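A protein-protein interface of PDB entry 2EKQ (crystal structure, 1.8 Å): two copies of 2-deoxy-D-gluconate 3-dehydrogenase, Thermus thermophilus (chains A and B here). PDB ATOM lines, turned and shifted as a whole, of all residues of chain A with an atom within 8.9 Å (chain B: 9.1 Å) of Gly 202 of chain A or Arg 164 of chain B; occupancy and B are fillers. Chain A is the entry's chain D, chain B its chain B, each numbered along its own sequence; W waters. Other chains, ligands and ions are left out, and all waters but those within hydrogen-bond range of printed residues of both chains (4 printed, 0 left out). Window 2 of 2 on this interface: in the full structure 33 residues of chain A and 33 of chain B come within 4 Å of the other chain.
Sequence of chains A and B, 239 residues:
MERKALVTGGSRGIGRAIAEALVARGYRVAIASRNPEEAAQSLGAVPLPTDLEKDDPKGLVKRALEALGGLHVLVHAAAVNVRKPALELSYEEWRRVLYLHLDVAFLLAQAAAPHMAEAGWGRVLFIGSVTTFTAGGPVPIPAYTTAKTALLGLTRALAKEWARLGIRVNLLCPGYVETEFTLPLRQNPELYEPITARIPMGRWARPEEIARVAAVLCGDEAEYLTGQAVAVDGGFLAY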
ATOM      1  N   TYR A 192     -33.871  -9.579  13.336  1.00  0.00           N
ATOM      2  CA  TYR A 192     -33.648  -9.010  14.660  1.00  0.00           C
ATOM      3  C   TYR A 192     -34.175  -9.885  15.794  1.00  0.00           C
ATOM      4  O   TYR A 192     -33.455 -10.166  16.751  1.00  0.00           O
ATOM      5  CB  TYR A 192     -34.281  -7.616  14.740  1.00  0.00           C
ATOM      6  CG  TYR A 192     -34.137  -6.946  16.090  1.00  0.00           C
ATOM      7  CD1 TYR A 192     -35.004  -7.251  17.141  1.00  0.00           C
ATOM      8  CD2 TYR A 192     -33.119  -6.021  16.324  1.00  0.00           C
ATOM      9  CE1 TYR A 192     -34.858  -6.653  18.391  1.00  0.00           C
ATOM     10  CE2 TYR A 192     -32.966  -5.420  17.570  1.00  0.00           C
ATOM     11  CZ  TYR A 192     -33.837  -5.741  18.597  1.00  0.00           C
ATOM     12  OH  TYR A 192     -33.685  -5.151  19.832  1.00  0.00           O
ATOM     13  N   GLU A 193     -35.429 -10.311  15.683  1.00  0.00           N
ATOM     14  CA  GLU A 193     -36.057 -11.137  16.712  1.00  0.00           C
ATOM     15  C   GLU A 193     -35.292 -12.417  17.054  1.00  0.00           C
ATOM     16  O   GLU A 193     -34.946 -12.645  18.213  1.00  0.00           O
ATOM     17  CB  GLU A 193     -37.491 -11.482  16.298  1.00  0.00           C
ATOM     18  CG  GLU A 193     -38.417 -10.277  16.226  1.00  0.00           C
ATOM     19  CD  GLU A 193     -38.676  -9.663  17.587  1.00  0.00           C
ATOM     20  OE1 GLU A 193     -39.265 -10.353  18.445  1.00  0.00           O
ATOM     21  OE2 GLU A 193     -38.289  -8.494  17.798  1.00  0.00           O
ATOM     22  N   ILE A 195     -32.211 -13.280  16.443  1.00  0.00           N
ATOM     23  CA  ILE A 195     -30.891 -12.941  16.958  1.00  0.00           C
ATOM     24  C   ILE A 195     -30.956 -12.423  18.392  1.00  0.00           C
ATOM     25  O   ILE A 195     -30.197 -12.863  19.255  1.00  0.00           O
ATOM     26  CB  ILE A 195     -30.210 -11.881  16.067  1.00  0.00           C
ATOM     27  CG1 ILE A 195     -29.888 -12.492  14.700  1.00  0.00           C
ATOM     28  CG2 ILE A 195     -28.948 -11.354  16.740  1.00  0.00           C
ATOM     29  CD1 ILE A 195     -29.256 -11.524  13.723  1.00  0.00           C
ATOM     30  N   THR A 196     -31.869 -11.492  18.643  1.00  0.00           N
ATOM     31  CA  THR A 196     -32.016 -10.917  19.973  1.00  0.00           C
ATOM     32  C   THR A 196     -32.428 -11.970  20.997  1.00  0.00           C
ATOM     33  O   THR A 196     -32.112 -11.853  22.180  1.00  0.00           O
ATOM     34  CB  THR A 196     -33.051  -9.773  19.964  1.00  0.00           C
ATOM     35  OG1 THR A 196     -32.657  -8.790  18.999  1.00  0.00           O
ATOM     36  CG2 THR A 196     -33.139  -9.114  21.335  1.00  0.00           C
ATOM     37  N   ALA A 197     -33.129 -13.004  20.539  1.00  0.00           N
ATOM     38  CA  ALA A 197     -33.577 -14.071  21.426  1.00  0.00           C
ATOM     39  C   ALA A 197     -32.387 -14.912  21.877  1.00  0.00           C
ATOM     40  O   ALA A 197     -32.459 -15.616  22.888  1.00  0.00           O
ATOM     41  CB  ALA A 197     -34.598 -14.945  20.714  1.00  0.00           C
ATOM     42  N   ARG A 198     -31.294 -14.830  21.126  1.00  0.00           N
ATOM     43  CA  ARG A 198     -30.085 -15.582  21.448  1.00  0.00           C
ATOM     44  C   ARG A 198     -29.128 -14.757  22.304  1.00  0.00           C
ATOM     45  O   ARG A 198     -28.043 -15.220  22.656  1.00  0.00           O
ATOM     46  CB  ARG A 198     -29.384 -16.033  20.167  1.00  0.00           C
ATOM     47  CG  ARG A 198     -30.158 -17.086  19.392  1.00  0.00           C
ATOM     48  CD  ARG A 198     -29.537 -17.335  18.031  1.00  0.00           C
ATOM     49  NE  ARG A 198     -28.148 -17.780  18.120  1.00  0.00           N
ATOM     50  CZ  ARG A 198     -27.352 -17.944  17.069  1.00  0.00           C
ATOM     51  NH1 ARG A 198     -27.808 -17.698  15.848  1.00  0.00           N
ATOM     52  NH2 ARG A 198     -26.102 -18.351  17.235  1.00  0.00           N
ATOM     53  N   ILE A 199     -29.532 -13.529  22.622  1.00  0.00           N
ATOM     54  CA  ILE A 199     -28.726 -12.650  23.462  1.00  0.00           C
ATOM     55  C   ILE A 199     -29.313 -12.704  24.869  1.00  0.00           C
ATOM     56  O   ILE A 199     -30.389 -12.164  25.123  1.00  0.00           O
ATOM     57  CB  ILE A 199     -28.764 -11.189  22.961  1.00  0.00           C
ATOM     58  CG1 ILE A 199     -28.281 -11.118  21.509  1.00  0.00           C
ATOM     59  CG2 ILE A 199     -27.874 -10.312  23.841  1.00  0.00           C
ATOM     60  CD1 ILE A 199     -28.377  -9.735  20.898  1.00  0.00           C
ATOM     61  N   PRO A 200     -28.616 -13.372  25.802  1.00  0.00           N
ATOM     62  CA  PRO A 200     -29.081 -13.494  27.185  1.00  0.00           C
ATOM     63  C   PRO A 200     -29.520 -12.176  27.814  1.00  0.00           C
ATOM     64  O   PRO A 200     -30.550 -12.120  28.491  1.00  0.00           O
ATOM     65  CB  PRO A 200     -27.879 -14.111  27.891  1.00  0.00           C
ATOM     66  CG  PRO A 200     -27.329 -15.015  26.833  1.00  0.00           C
ATOM     67  CD  PRO A 200     -27.365 -14.127  25.605  1.00  0.00           C
ATOM     68  N   MET A 201     -28.754 -11.115  27.585  1.00  0.00           N
ATOM     69  CA  MET A 201     -29.093  -9.817  28.155  1.00  0.00           C
ATOM     70  C   MET A 201     -30.373  -9.221  27.574  1.00  0.00           C
ATOM     71  O   MET A 201     -30.946  -8.294  28.147  1.00  0.00           O
ATOM     72  CB  MET A 201     -27.918  -8.853  28.005  1.00  0.00           C
ATOM     73  CG  MET A 201     -26.843  -9.095  29.066  1.00  0.00           C
ATOM     74  SD  MET A 201     -25.442  -7.983  28.956  1.00  0.00           S
ATOM     75  CE  MET A 201     -26.254  -6.406  29.260  1.00  0.00           C
ATOM     76  N   GLY A 202     -30.813  -9.755  26.438  1.00  0.00           N
ATOM     77  CA  GLY A 202     -32.054  -9.297  25.833  1.00  0.00           C
ATOM     78  C   GLY A 202     -32.070  -7.969  25.101  1.00  0.00           C
ATOM     79  O   GLY A 202     -33.147  -7.467  24.767  1.00  0.00           O
ATOM     80  N   ARG A 203     -30.898  -7.396  24.856  1.00  0.00           N
ATOM     81  CA  ARG A 203     -30.809  -6.121  24.147  1.00  0.00           C
ATOM     82  C   ARG A 203     -29.482  -6.035  23.418  1.00  0.00           C
ATOM     83  O   ARG A 203     -28.552  -6.784  23.717  1.00  0.00           O
ATOM     84  CB  ARG A 203     -30.905  -4.944  25.124  1.00  0.00           C
ATOM     85  CG  ARG A 203     -29.710  -4.816  26.070  1.00  0.00           C
ATOM     86  CD  ARG A 203     -29.782  -3.530  26.883  1.00  0.00           C
ATOM     87  NE  ARG A 203     -28.725  -3.434  27.891  1.00  0.00           N
ATOM     88  CZ  ARG A 203     -27.456  -3.132  27.635  1.00  0.00           C
ATOM     89  NH1 ARG A 203     -27.058  -2.888  26.394  1.00  0.00           N
ATOM     90  NH2 ARG A 203     -26.579  -3.071  28.630  1.00  0.00           N
ATOM     91  N   TRP A 204     -29.396  -5.120  22.459  1.00  0.00           N
ATOM     92  CA  TRP A 204     -28.163  -4.926  21.713  1.00  0.00           C
ATOM     93  C   TRP A 204     -27.266  -4.005  22.532  1.00  0.00           C
ATOM     94  O   TRP A 204     -27.724  -3.362  23.480  1.00  0.00           O
ATOM     95  CB  TRP A 204     -28.469  -4.323  20.338  1.00  0.00           C
ATOM     96  CG  TRP A 204     -29.025  -5.334  19.370  1.00  0.00           C
ATOM     97  CD1 TRP A 204     -29.930  -6.320  19.643  1.00  0.00           C
ATOM     98  CD2 TRP A 204     -28.699  -5.465  17.981  1.00  0.00           C
ATOM     99  NE1 TRP A 204     -30.186  -7.058  18.513  1.00  0.00           N
ATOM    100  CE2 TRP A 204     -29.445  -6.554  17.476  1.00  0.00           C
ATOM    101  CE3 TRP A 204     -27.849  -4.767  17.111  1.00  0.00           C
ATOM    102  CZ2 TRP A 204     -29.366  -6.964  16.141  1.00  0.00           C
ATOM    103  CZ3 TRP A 204     -27.770  -5.174  15.784  1.00  0.00           C
ATOM    104  CH2 TRP A 204     -28.527  -6.264  15.313  1.00  0.00           C
ATOM    105  N   ALA A 205     -25.991  -3.942  22.174  1.00  0.00           N
ATOM    106  CA  ALA A 205     -25.048  -3.113  22.906  1.00  0.00           C
ATOM    107  C   ALA A 205     -24.991  -1.682  22.406  1.00  0.00           C
ATOM    108  O   ALA A 205     -25.344  -1.396  21.265  1.00  0.00           O
ATOM    109  CB  ALA A 205     -23.656  -3.725  22.829  1.00  0.00           C
ATOM    110  N   ASP A 233     -20.387  -9.577  23.878  1.00  0.00           N
ATOM    111  CA  ASP A 233     -21.634  -9.815  23.159  1.00  0.00           C
ATOM    112  C   ASP A 233     -22.906 -10.042  23.973  1.00  0.00           C
ATOM    113  O   ASP A 233     -23.849 -10.644  23.468  1.00  0.00           O
ATOM    114  CB  ASP A 233     -21.438 -11.024  22.241  1.00  0.00           C
ATOM    115  CG  ASP A 233     -21.193 -12.312  23.020  1.00  0.00           C
ATOM    116  OD1 ASP A 233     -21.195 -12.272  24.272  1.00  0.00           O
ATOM    117  OD2 ASP A 233     -21.002 -13.370  22.389  1.00  0.00           O
ATOM    118  N   GLY A 234     -22.938  -9.586  25.220  1.00  0.00           N
ATOM    119  CA  GLY A 234     -24.134  -9.768  26.026  1.00  0.00           C
ATOM    120  C   GLY A 234     -24.515 -11.220  26.255  1.00  0.00           C
ATOM    121  O   GLY A 234     -25.654 -11.512  26.634  1.00  0.00           O
ATOM    122  N   GLY A 235     -23.569 -12.127  26.022  1.00  0.00           N
ATOM    123  CA  GLY A 235     -23.819 -13.548  26.221  1.00  0.00           C
ATOM    124  C   GLY A 235     -24.230 -14.333  24.987  1.00  0.00           C
ATOM    125  O   GLY A 235     -24.506 -15.530  25.080  1.00  0.00           O
ATOM    126  N   PHE A 236     -24.263 -13.672  23.832  1.00  0.00           N
ATOM    127  CA  PHE A 236     -24.670 -14.304  22.575  1.00  0.00           C
ATOM    128  C   PHE A 236     -23.963 -15.618  22.237  1.00  0.00           C
ATOM    129  O   PHE A 236     -24.615 -16.626  21.960  1.00  0.00           O
ATOM    130  CB  PHE A 236     -24.476 -13.330  21.409  1.00  0.00           C
ATOM    131  CG  PHE A 236     -24.892 -13.892  20.074  1.00  0.00           C
ATOM    132  CD1 PHE A 236     -26.236 -13.938  19.714  1.00  0.00           C
ATOM    133  CD2 PHE A 236     -23.943 -14.390  19.186  1.00  0.00           C
ATOM    134  CE1 PHE A 236     -26.632 -14.473  18.484  1.00  0.00           C
ATOM    135  CE2 PHE A 236     -24.327 -14.928  17.956  1.00  0.00           C
ATOM    136  CZ  PHE A 236     -25.676 -14.968  17.607  1.00  0.00           C
ATOM    137  N   TYR A 239     -24.800 -18.515  24.773  1.00  0.00           N
ATOM    138  CA  TYR A 239     -26.176 -19.008  24.717  1.00  0.00           C
ATOM    139  C   TYR A 239     -26.308 -20.496  24.390  1.00  0.00           C
ATOM    140  O   TYR A 239     -25.970 -20.886  23.255  1.00  0.00           O
ATOM    141  CB  TYR A 239     -26.974 -18.189  23.701  1.00  0.00           C
ATOM    142  CG  TYR A 239     -28.460 -18.478  23.695  1.00  0.00           C
ATOM    143  CD1 TYR A 239     -29.259 -18.162  24.797  1.00  0.00           C
ATOM    144  CD2 TYR A 239     -29.069 -19.056  22.584  1.00  0.00           C
ATOM    145  CE1 TYR A 239     -30.633 -18.416  24.787  1.00  0.00           C
ATOM    146  CE2 TYR A 239     -30.437 -19.311  22.564  1.00  0.00           C
ATOM    147  CZ  TYR A 239     -31.212 -18.988  23.665  1.00  0.00           C
ATOM    148  OH  TYR A 239     -32.566 -19.227  23.632  1.00  0.00           O
ATOM    149  OXT TYR A 239     -26.753 -21.254  25.277  1.00  0.00           O
ATOM    150  N   MET B 116     -27.222 -10.661  44.488  1.00  0.00           N
ATOM    151  CA  MET B 116     -26.808  -9.793  43.397  1.00  0.00           C
ATOM    152  C   MET B 116     -28.057  -9.356  42.640  1.00  0.00           C
ATOM    153  O   MET B 116     -28.185  -8.196  42.252  1.00  0.00           O
ATOM    154  CB  MET B 116     -25.869 -10.536  42.449  1.00  0.00           C
ATOM    155  CG  MET B 116     -24.594 -11.027  43.107  1.00  0.00           C
ATOM    156  SD  MET B 116     -23.615 -12.058  41.996  1.00  0.00           S
ATOM    157  CE  MET B 116     -22.029 -12.036  42.845  1.00  0.00           C
ATOM    158  N   ALA B 117     -28.974 -10.296  42.442  1.00  0.00           N
ATOM    159  CA  ALA B 117     -30.212 -10.022  41.732  1.00  0.00           C
ATOM    160  C   ALA B 117     -31.034  -8.955  42.444  1.00  0.00           C
ATOM    161  O   ALA B 117     -31.638  -8.102  41.800  1.00  0.00           O
ATOM    162  CB  ALA B 117     -31.029 -11.305  41.586  1.00  0.00           C
ATOM    163  N   GLY B 120     -29.623  -5.823  41.704  1.00  0.00           N
ATOM    164  CA  GLY B 120     -29.773  -5.529  40.290  1.00  0.00           C
ATOM    165  C   GLY B 120     -28.441  -5.373  39.578  1.00  0.00           C
ATOM    166  O   GLY B 120     -28.371  -4.841  38.469  1.00  0.00           O
ATOM    167  N   TRP B 121     -27.376  -5.847  40.212  1.00  0.00           N
ATOM    168  CA  TRP B 121     -26.039  -5.742  39.646  1.00  0.00           C
ATOM    169  C   TRP B 121     -25.161  -6.785  40.313  1.00  0.00           C
ATOM    170  O   TRP B 121     -25.134  -6.888  41.539  1.00  0.00           O
ATOM    171  CB  TRP B 121     -25.477  -4.348  39.921  1.00  0.00           C
ATOM    172  CG  TRP B 121     -24.209  -4.013  39.195  1.00  0.00           C
ATOM    173  CD1 TRP B 121     -24.091  -3.286  38.046  1.00  0.00           C
ATOM    174  CD2 TRP B 121     -22.874  -4.343  39.599  1.00  0.00           C
ATOM    175  NE1 TRP B 121     -22.766  -3.133  37.712  1.00  0.00           N
ATOM    176  CE2 TRP B 121     -21.996  -3.774  38.649  1.00  0.00           C
ATOM    177  CE3 TRP B 121     -22.334  -5.064  40.674  1.00  0.00           C
ATOM    178  CZ2 TRP B 121     -20.607  -3.899  38.741  1.00  0.00           C
ATOM    179  CZ3 TRP B 121     -20.947  -5.188  40.766  1.00  0.00           C
ATOM    180  CH2 TRP B 121     -20.102  -4.607  39.803  1.00  0.00           C
ATOM    181  N   LEU B 158     -24.345 -20.248  33.698  1.00  0.00           N
ATOM    182  CA  LEU B 158     -24.823 -19.256  34.653  1.00  0.00           C
ATOM    183  C   LEU B 158     -24.954 -17.884  34.002  1.00  0.00           C
ATOM    184  O   LEU B 158     -25.859 -17.115  34.340  1.00  0.00           O
ATOM    185  CB  LEU B 158     -23.889 -19.189  35.868  1.00  0.00           C
ATOM    186  CG  LEU B 158     -23.723 -20.517  36.620  1.00  0.00           C
ATOM    187  CD1 LEU B 158     -22.896 -20.291  37.880  1.00  0.00           C
ATOM    188  CD2 LEU B 158     -25.094 -21.091  36.980  1.00  0.00           C
ATOM    189  N   ALA B 159     -24.062 -17.572  33.066  1.00  0.00           N
ATOM    190  CA  ALA B 159     -24.131 -16.284  32.382  1.00  0.00           C
ATOM    191  C   ALA B 159     -25.455 -16.202  31.632  1.00  0.00           C
ATOM    192  O   ALA B 159     -26.126 -15.175  31.656  1.00  0.00           O
ATOM    193  CB  ALA B 159     -22.970 -16.134  31.411  1.00  0.00           C
ATOM    194  N   LYS B 160     -25.835 -17.296  30.980  1.00  0.00           N
ATOM    195  CA  LYS B 160     -27.085 -17.332  30.226  1.00  0.00           C
ATOM    196  C   LYS B 160     -28.304 -17.173  31.136  1.00  0.00           C
ATOM    197  O   LYS B 160     -29.224 -16.411  30.838  1.00  0.00           O
ATOM    198  CB  LYS B 160     -27.211 -18.658  29.467  1.00  0.00           C
ATOM    199  CG  LYS B 160     -28.448 -18.748  28.573  1.00  0.00           C
ATOM    200  CD  LYS B 160     -28.690 -20.166  28.052  1.00  0.00           C
ATOM    201  CE  LYS B 160     -29.185 -21.089  29.155  1.00  0.00           C
ATOM    202  NZ  LYS B 160     -29.534 -22.445  28.642  1.00  0.00           N
ATOM    203  N   GLU B 161     -28.306 -17.907  32.242  1.00  0.00           N
ATOM    204  CA  GLU B 161     -29.414 -17.890  33.188  1.00  0.00           C
ATOM    205  C   GLU B 161     -29.607 -16.587  33.960  1.00  0.00           C
ATOM    206  O   GLU B 161     -30.738 -16.167  34.206  1.00  0.00           O
ATOM    207  CB  GLU B 161     -29.239 -19.045  34.182  1.00  0.00           C
ATOM    208  CG  GLU B 161     -30.437 -19.303  35.080  1.00  0.00           C
ATOM    209  CD  GLU B 161     -30.194 -20.476  36.020  1.00  0.00           C
ATOM    210  OE1 GLU B 161     -29.660 -21.505  35.549  1.00  0.00           O
ATOM    211  OE2 GLU B 161     -30.539 -20.378  37.220  1.00  0.00           O
ATOM    212  N   TRP B 162     -28.509 -15.939  34.327  1.00  0.00           N
ATOM    213  CA  TRP B 162     -28.604 -14.731  35.137  1.00  0.00           C
ATOM    214  C   TRP B 162     -28.405 -13.384  34.445  1.00  0.00           C
ATOM    215  O   TRP B 162     -28.411 -12.346  35.106  1.00  0.00           O
ATOM    216  CB  TRP B 162     -27.632 -14.854  36.319  1.00  0.00           C
ATOM    217  CG  TRP B 162     -27.865 -16.098  37.137  1.00  0.00           C
ATOM    218  CD1 TRP B 162     -29.033 -16.801  37.239  1.00  0.00           C
ATOM    219  CD2 TRP B 162     -26.923 -16.763  37.991  1.00  0.00           C
ATOM    220  NE1 TRP B 162     -28.878 -17.860  38.101  1.00  0.00           N
ATOM    221  CE2 TRP B 162     -27.594 -17.860  38.577  1.00  0.00           C
ATOM    222  CE3 TRP B 162     -25.579 -16.537  38.322  1.00  0.00           C
ATOM    223  CZ2 TRP B 162     -26.968 -18.732  39.473  1.00  0.00           C
ATOM    224  CZ3 TRP B 162     -24.954 -17.406  39.217  1.00  0.00           C
ATOM    225  CH2 TRP B 162     -25.652 -18.491  39.780  1.00  0.00           C
ATOM    226  N   ALA B 163     -28.254 -13.388  33.125  1.00  0.00           N
ATOM    227  CA  ALA B 163     -28.044 -12.142  32.391  1.00  0.00           C
ATOM    228  C   ALA B 163     -29.120 -11.090  32.663  1.00  0.00           C
ATOM    229  O   ALA B 163     -28.806  -9.926  32.917  1.00  0.00           O
ATOM    230  CB  ALA B 163     -27.960 -12.429  30.898  1.00  0.00           C
ATOM    231  N   ARG B 164     -30.386 -11.497  32.610  1.00  0.00           N
ATOM    232  CA  ARG B 164     -31.493 -10.568  32.844  1.00  0.00           C
ATOM    233  C   ARG B 164     -31.539 -10.029  34.273  1.00  0.00           C
ATOM    234  O   ARG B 164     -32.195  -9.020  34.537  1.00  0.00           O
ATOM    235  CB  ARG B 164     -32.838 -11.232  32.522  1.00  0.00           C
ATOM    236  CG  ARG B 164     -33.043 -11.625  31.064  1.00  0.00           C
ATOM    237  CD  ARG B 164     -32.912 -10.444  30.110  1.00  0.00           C
ATOM    238  NE  ARG B 164     -33.326 -10.799  28.750  1.00  0.00           N
ATOM    239  CZ  ARG B 164     -34.581 -10.754  28.311  1.00  0.00           C
ATOM    240  NH1 ARG B 164     -35.560 -10.363  29.116  1.00  0.00           N
ATOM    241  NH2 ARG B 164     -34.861 -11.105  27.061  1.00  0.00           N
ATOM    242  N   LEU B 165     -30.851 -10.702  35.193  1.00  0.00           N
ATOM    243  CA  LEU B 165     -30.829 -10.286  36.593  1.00  0.00           C
ATOM    244  C   LEU B 165     -29.813  -9.184  36.851  1.00  0.00           C
ATOM    245  O   LEU B 165     -29.778  -8.608  37.944  1.00  0.00           O
ATOM    246  CB  LEU B 165     -30.512 -11.485  37.495  1.00  0.00           C
ATOM    247  CG  LEU B 165     -31.453 -12.687  37.386  1.00  0.00           C
ATOM    248  CD1 LEU B 165     -30.976 -13.807  38.307  1.00  0.00           C
ATOM    249  CD2 LEU B 165     -32.870 -12.260  37.754  1.00  0.00           C
ATOM    250  N   GLY B 166     -28.991  -8.893  35.846  1.00  0.00           N
ATOM    251  CA  GLY B 166     -27.979  -7.861  35.986  1.00  0.00           C
ATOM    252  C   GLY B 166     -26.644  -8.447  36.402  1.00  0.00           C
ATOM    253  O   GLY B 166     -25.714  -7.724  36.759  1.00  0.00           O
ATOM    254  N   ILE B 167     -26.551  -9.771  36.350  1.00  0.00           N
ATOM    255  CA  ILE B 167     -25.329 -10.471  36.733  1.00  0.00           C
ATOM    256  C   ILE B 167     -24.518 -10.902  35.518  1.00  0.00           C
ATOM    257  O   ILE B 167     -25.066 -11.411  34.539  1.00  0.00           O
ATOM    258  CB  ILE B 167     -25.655 -11.731  37.567  1.00  0.00           C
ATOM    259  CG1 ILE B 167     -26.458 -11.345  38.813  1.00  0.00           C
ATOM    260  CG2 ILE B 167     -24.365 -12.440  37.962  1.00  0.00           C
ATOM    261  CD1 ILE B 167     -26.950 -12.538  39.617  1.00  0.00           C
ATOM    262  N   ARG B 168     -23.210 -10.683  35.583  1.00  0.00           N
ATOM    263  CA  ARG B 168     -22.310 -11.079  34.510  1.00  0.00           C
ATOM    264  C   ARG B 168     -21.429 -12.170  35.109  1.00  0.00           C
ATOM    265  O   ARG B 168     -20.946 -12.029  36.235  1.00  0.00           O
ATOM    266  CB  ARG B 168     -21.450  -9.893  34.064  1.00  0.00           C
ATOM    267  CG  ARG B 168     -22.256  -8.644  33.722  1.00  0.00           C
ATOM    268  CD  ARG B 168     -23.202  -8.887  32.550  1.00  0.00           C
ATOM    269  NE  ARG B 168     -24.105  -7.756  32.343  1.00  0.00           N
ATOM    270  CZ  ARG B 168     -25.402  -7.765  32.636  1.00  0.00           C
ATOM    271  NH1 ARG B 168     -25.959  -8.851  33.149  1.00  0.00           N
ATOM    272  NH2 ARG B 168     -26.142  -6.686  32.417  1.00  0.00           N
ATOM    273  N   GLU B 223     -20.014  -4.601  31.617  1.00  0.00           N
ATOM    274  CA  GLU B 223     -21.461  -4.446  31.519  1.00  0.00           C
ATOM    275  C   GLU B 223     -22.100  -5.272  30.399  1.00  0.00           C
ATOM    276  O   GLU B 223     -23.211  -5.780  30.556  1.00  0.00           O
ATOM    277  CB  GLU B 223     -21.817  -2.966  31.351  1.00  0.00           C
ATOM    278  CG  GLU B 223     -23.309  -2.713  31.243  1.00  0.00           C
ATOM    279  CD  GLU B 223     -24.100  -3.580  32.198  1.00  0.00           C
ATOM    280  OE1 GLU B 223     -23.808  -3.545  33.406  1.00  0.00           O
ATOM    281  OE2 GLU B 223     -25.010  -4.303  31.743  1.00  0.00           O
ATOM    282  N   TYR B 224     -21.406  -5.416  29.274  1.00  0.00           N
ATOM    283  CA  TYR B 224     -21.944  -6.196  28.161  1.00  0.00           C
ATOM    284  C   TYR B 224     -21.048  -7.398  27.874  1.00  0.00           C
ATOM    285  O   TYR B 224     -21.098  -7.979  26.788  1.00  0.00           O
ATOM    286  CB  TYR B 224     -22.053  -5.328  26.900  1.00  0.00           C
ATOM    287  CG  TYR B 224     -23.081  -5.822  25.898  1.00  0.00           C
ATOM    288  CD1 TYR B 224     -24.448  -5.733  26.172  1.00  0.00           C
ATOM    289  CD2 TYR B 224     -22.687  -6.378  24.679  1.00  0.00           C
ATOM    290  CE1 TYR B 224     -25.402  -6.187  25.254  1.00  0.00           C
ATOM    291  CE2 TYR B 224     -23.634  -6.834  23.752  1.00  0.00           C
ATOM    292  CZ  TYR B 224     -24.989  -6.733  24.049  1.00  0.00           C
ATOM    293  OH  TYR B 224     -25.932  -7.169  23.139  1.00  0.00           O
ATOM    294  N   THR B 226     -20.194 -11.129  29.110  1.00  0.00           N
ATOM    295  CA  THR B 226     -20.600 -12.236  29.964  1.00  0.00           C
ATOM    296  C   THR B 226     -20.572 -13.590  29.254  1.00  0.00           C
ATOM    297  O   THR B 226     -20.741 -13.668  28.034  1.00  0.00           O
ATOM    298  CB  THR B 226     -22.014 -11.968  30.542  1.00  0.00           C
ATOM    299  OG1 THR B 226     -22.260 -12.851  31.644  1.00  0.00           O
ATOM    300  CG2 THR B 226     -23.085 -12.178  29.472  1.00  0.00           C
HETATM  301  O   HOH W   1     -20.832 -14.824  25.456  1.00  0.00           O
HETATM  302  O   HOH W   2     -24.791  -9.162  21.308  1.00  0.00           O
HETATM  303  O   HOH W   3     -19.457 -11.200  26.230  1.00  0.00           O
HETATM  304  O   HOH W   4     -33.489 -12.085  24.594  1.00  0.00           O
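NE of Arg 164 of chain B is in hydrogen-bond range of O of Pro 200 of chain A (3.1 Å). OE2 of Glu 223 of chain B is in salt-bridge range of NH2 of Arg 203 of chain A (3.7 Å). N of Gly 234 of chain A lies within hydrogen-bond range of O of Tyr 224 of chain B, at 2.9 Å. The backbone carbonyl oxygen (O) of Tyr 224 of chain B sits at hydrogen-bond distance from the backbone NH (N) of Asp 233 of chain A. The side-chain hydroxyl (OH) of Tyr 224 of chain B lies within hydrogen-bond range of the backbone carbonyl oxygen (O) of Arg 203 of chain A, 2.7 Å away. The backbone carbonyl oxygen of Glu 223 of chain B sits close to the side-chain sulfur of Met 201 of chain A (3.5 Å). The backbone NH (N) of Ala 205 of chain A lies within hydrogen-bond range of the side-chain hydroxyl (OH) of Tyr 224 of chain B, 3.4 Å away. The guanidinium group of Arg 168 of chain B lies within hydrogen-bond range of the side-chain sulfur of Met 201 of chain A (3.6 Å).
OG1 of Thr 196 of chain A sits at hydrogen-bond distance from NE1 of Trp 204 of chain A, 3.1 Å away. The side-chain carboxylate of Glu 223 of chain B is in salt-bridge range of the guanidinium group of Arg 168 of chain B.
Of the printed residues of chain B, Met 201 of chain A touches Ala 163 (3.7 Å), Arg 164 (3.5 Å), Arg 168 (3.2 Å), Glu 223 (3.4 Å) and Tyr 224 (3.6 Å). Gly 202 of chain A touches one residue of chain B. Printed residues of chain A within 4 Å of Lys 160 of chain B: Pro 200 and Tyr 239. Arg 164 of chain B touches three residues of chain A. The nearest printed residue of chain B that does not touch Gly 235 of chain A is Tyr 224 of chain B (4.9 Å).
Along chain B the printed residues that touch a printed residue of chain A span positions 160 to 226. Printed residues of chain A that touch a printed residue of chain B: Ile 199, Pro 200, Met 201, Gly 202, Arg 203, Trp 204, Ala 205, Asp 233, Gly 234, Gly 235 and Tyr 239. Hydrophobic or aromatic side chains of chain A that line the printed part of chain B: Ile 199, Pro 200, Met 201, Ala 205 and Tyr 239. Among the printed residues, 19 pairs touch across the chains.
No position is printed for both chains. Of the 19 pairs that touch across the chains among the printed residues, none has its exchanged pair printed and touching as well.
Water W4 lies within hydrogen-bond range of O of Thr 196 of chain A (2.8 Å), NH2 of Arg 164 of chain B (3.0 Å) and O of Ile 199 of chain A (3.1 Å).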
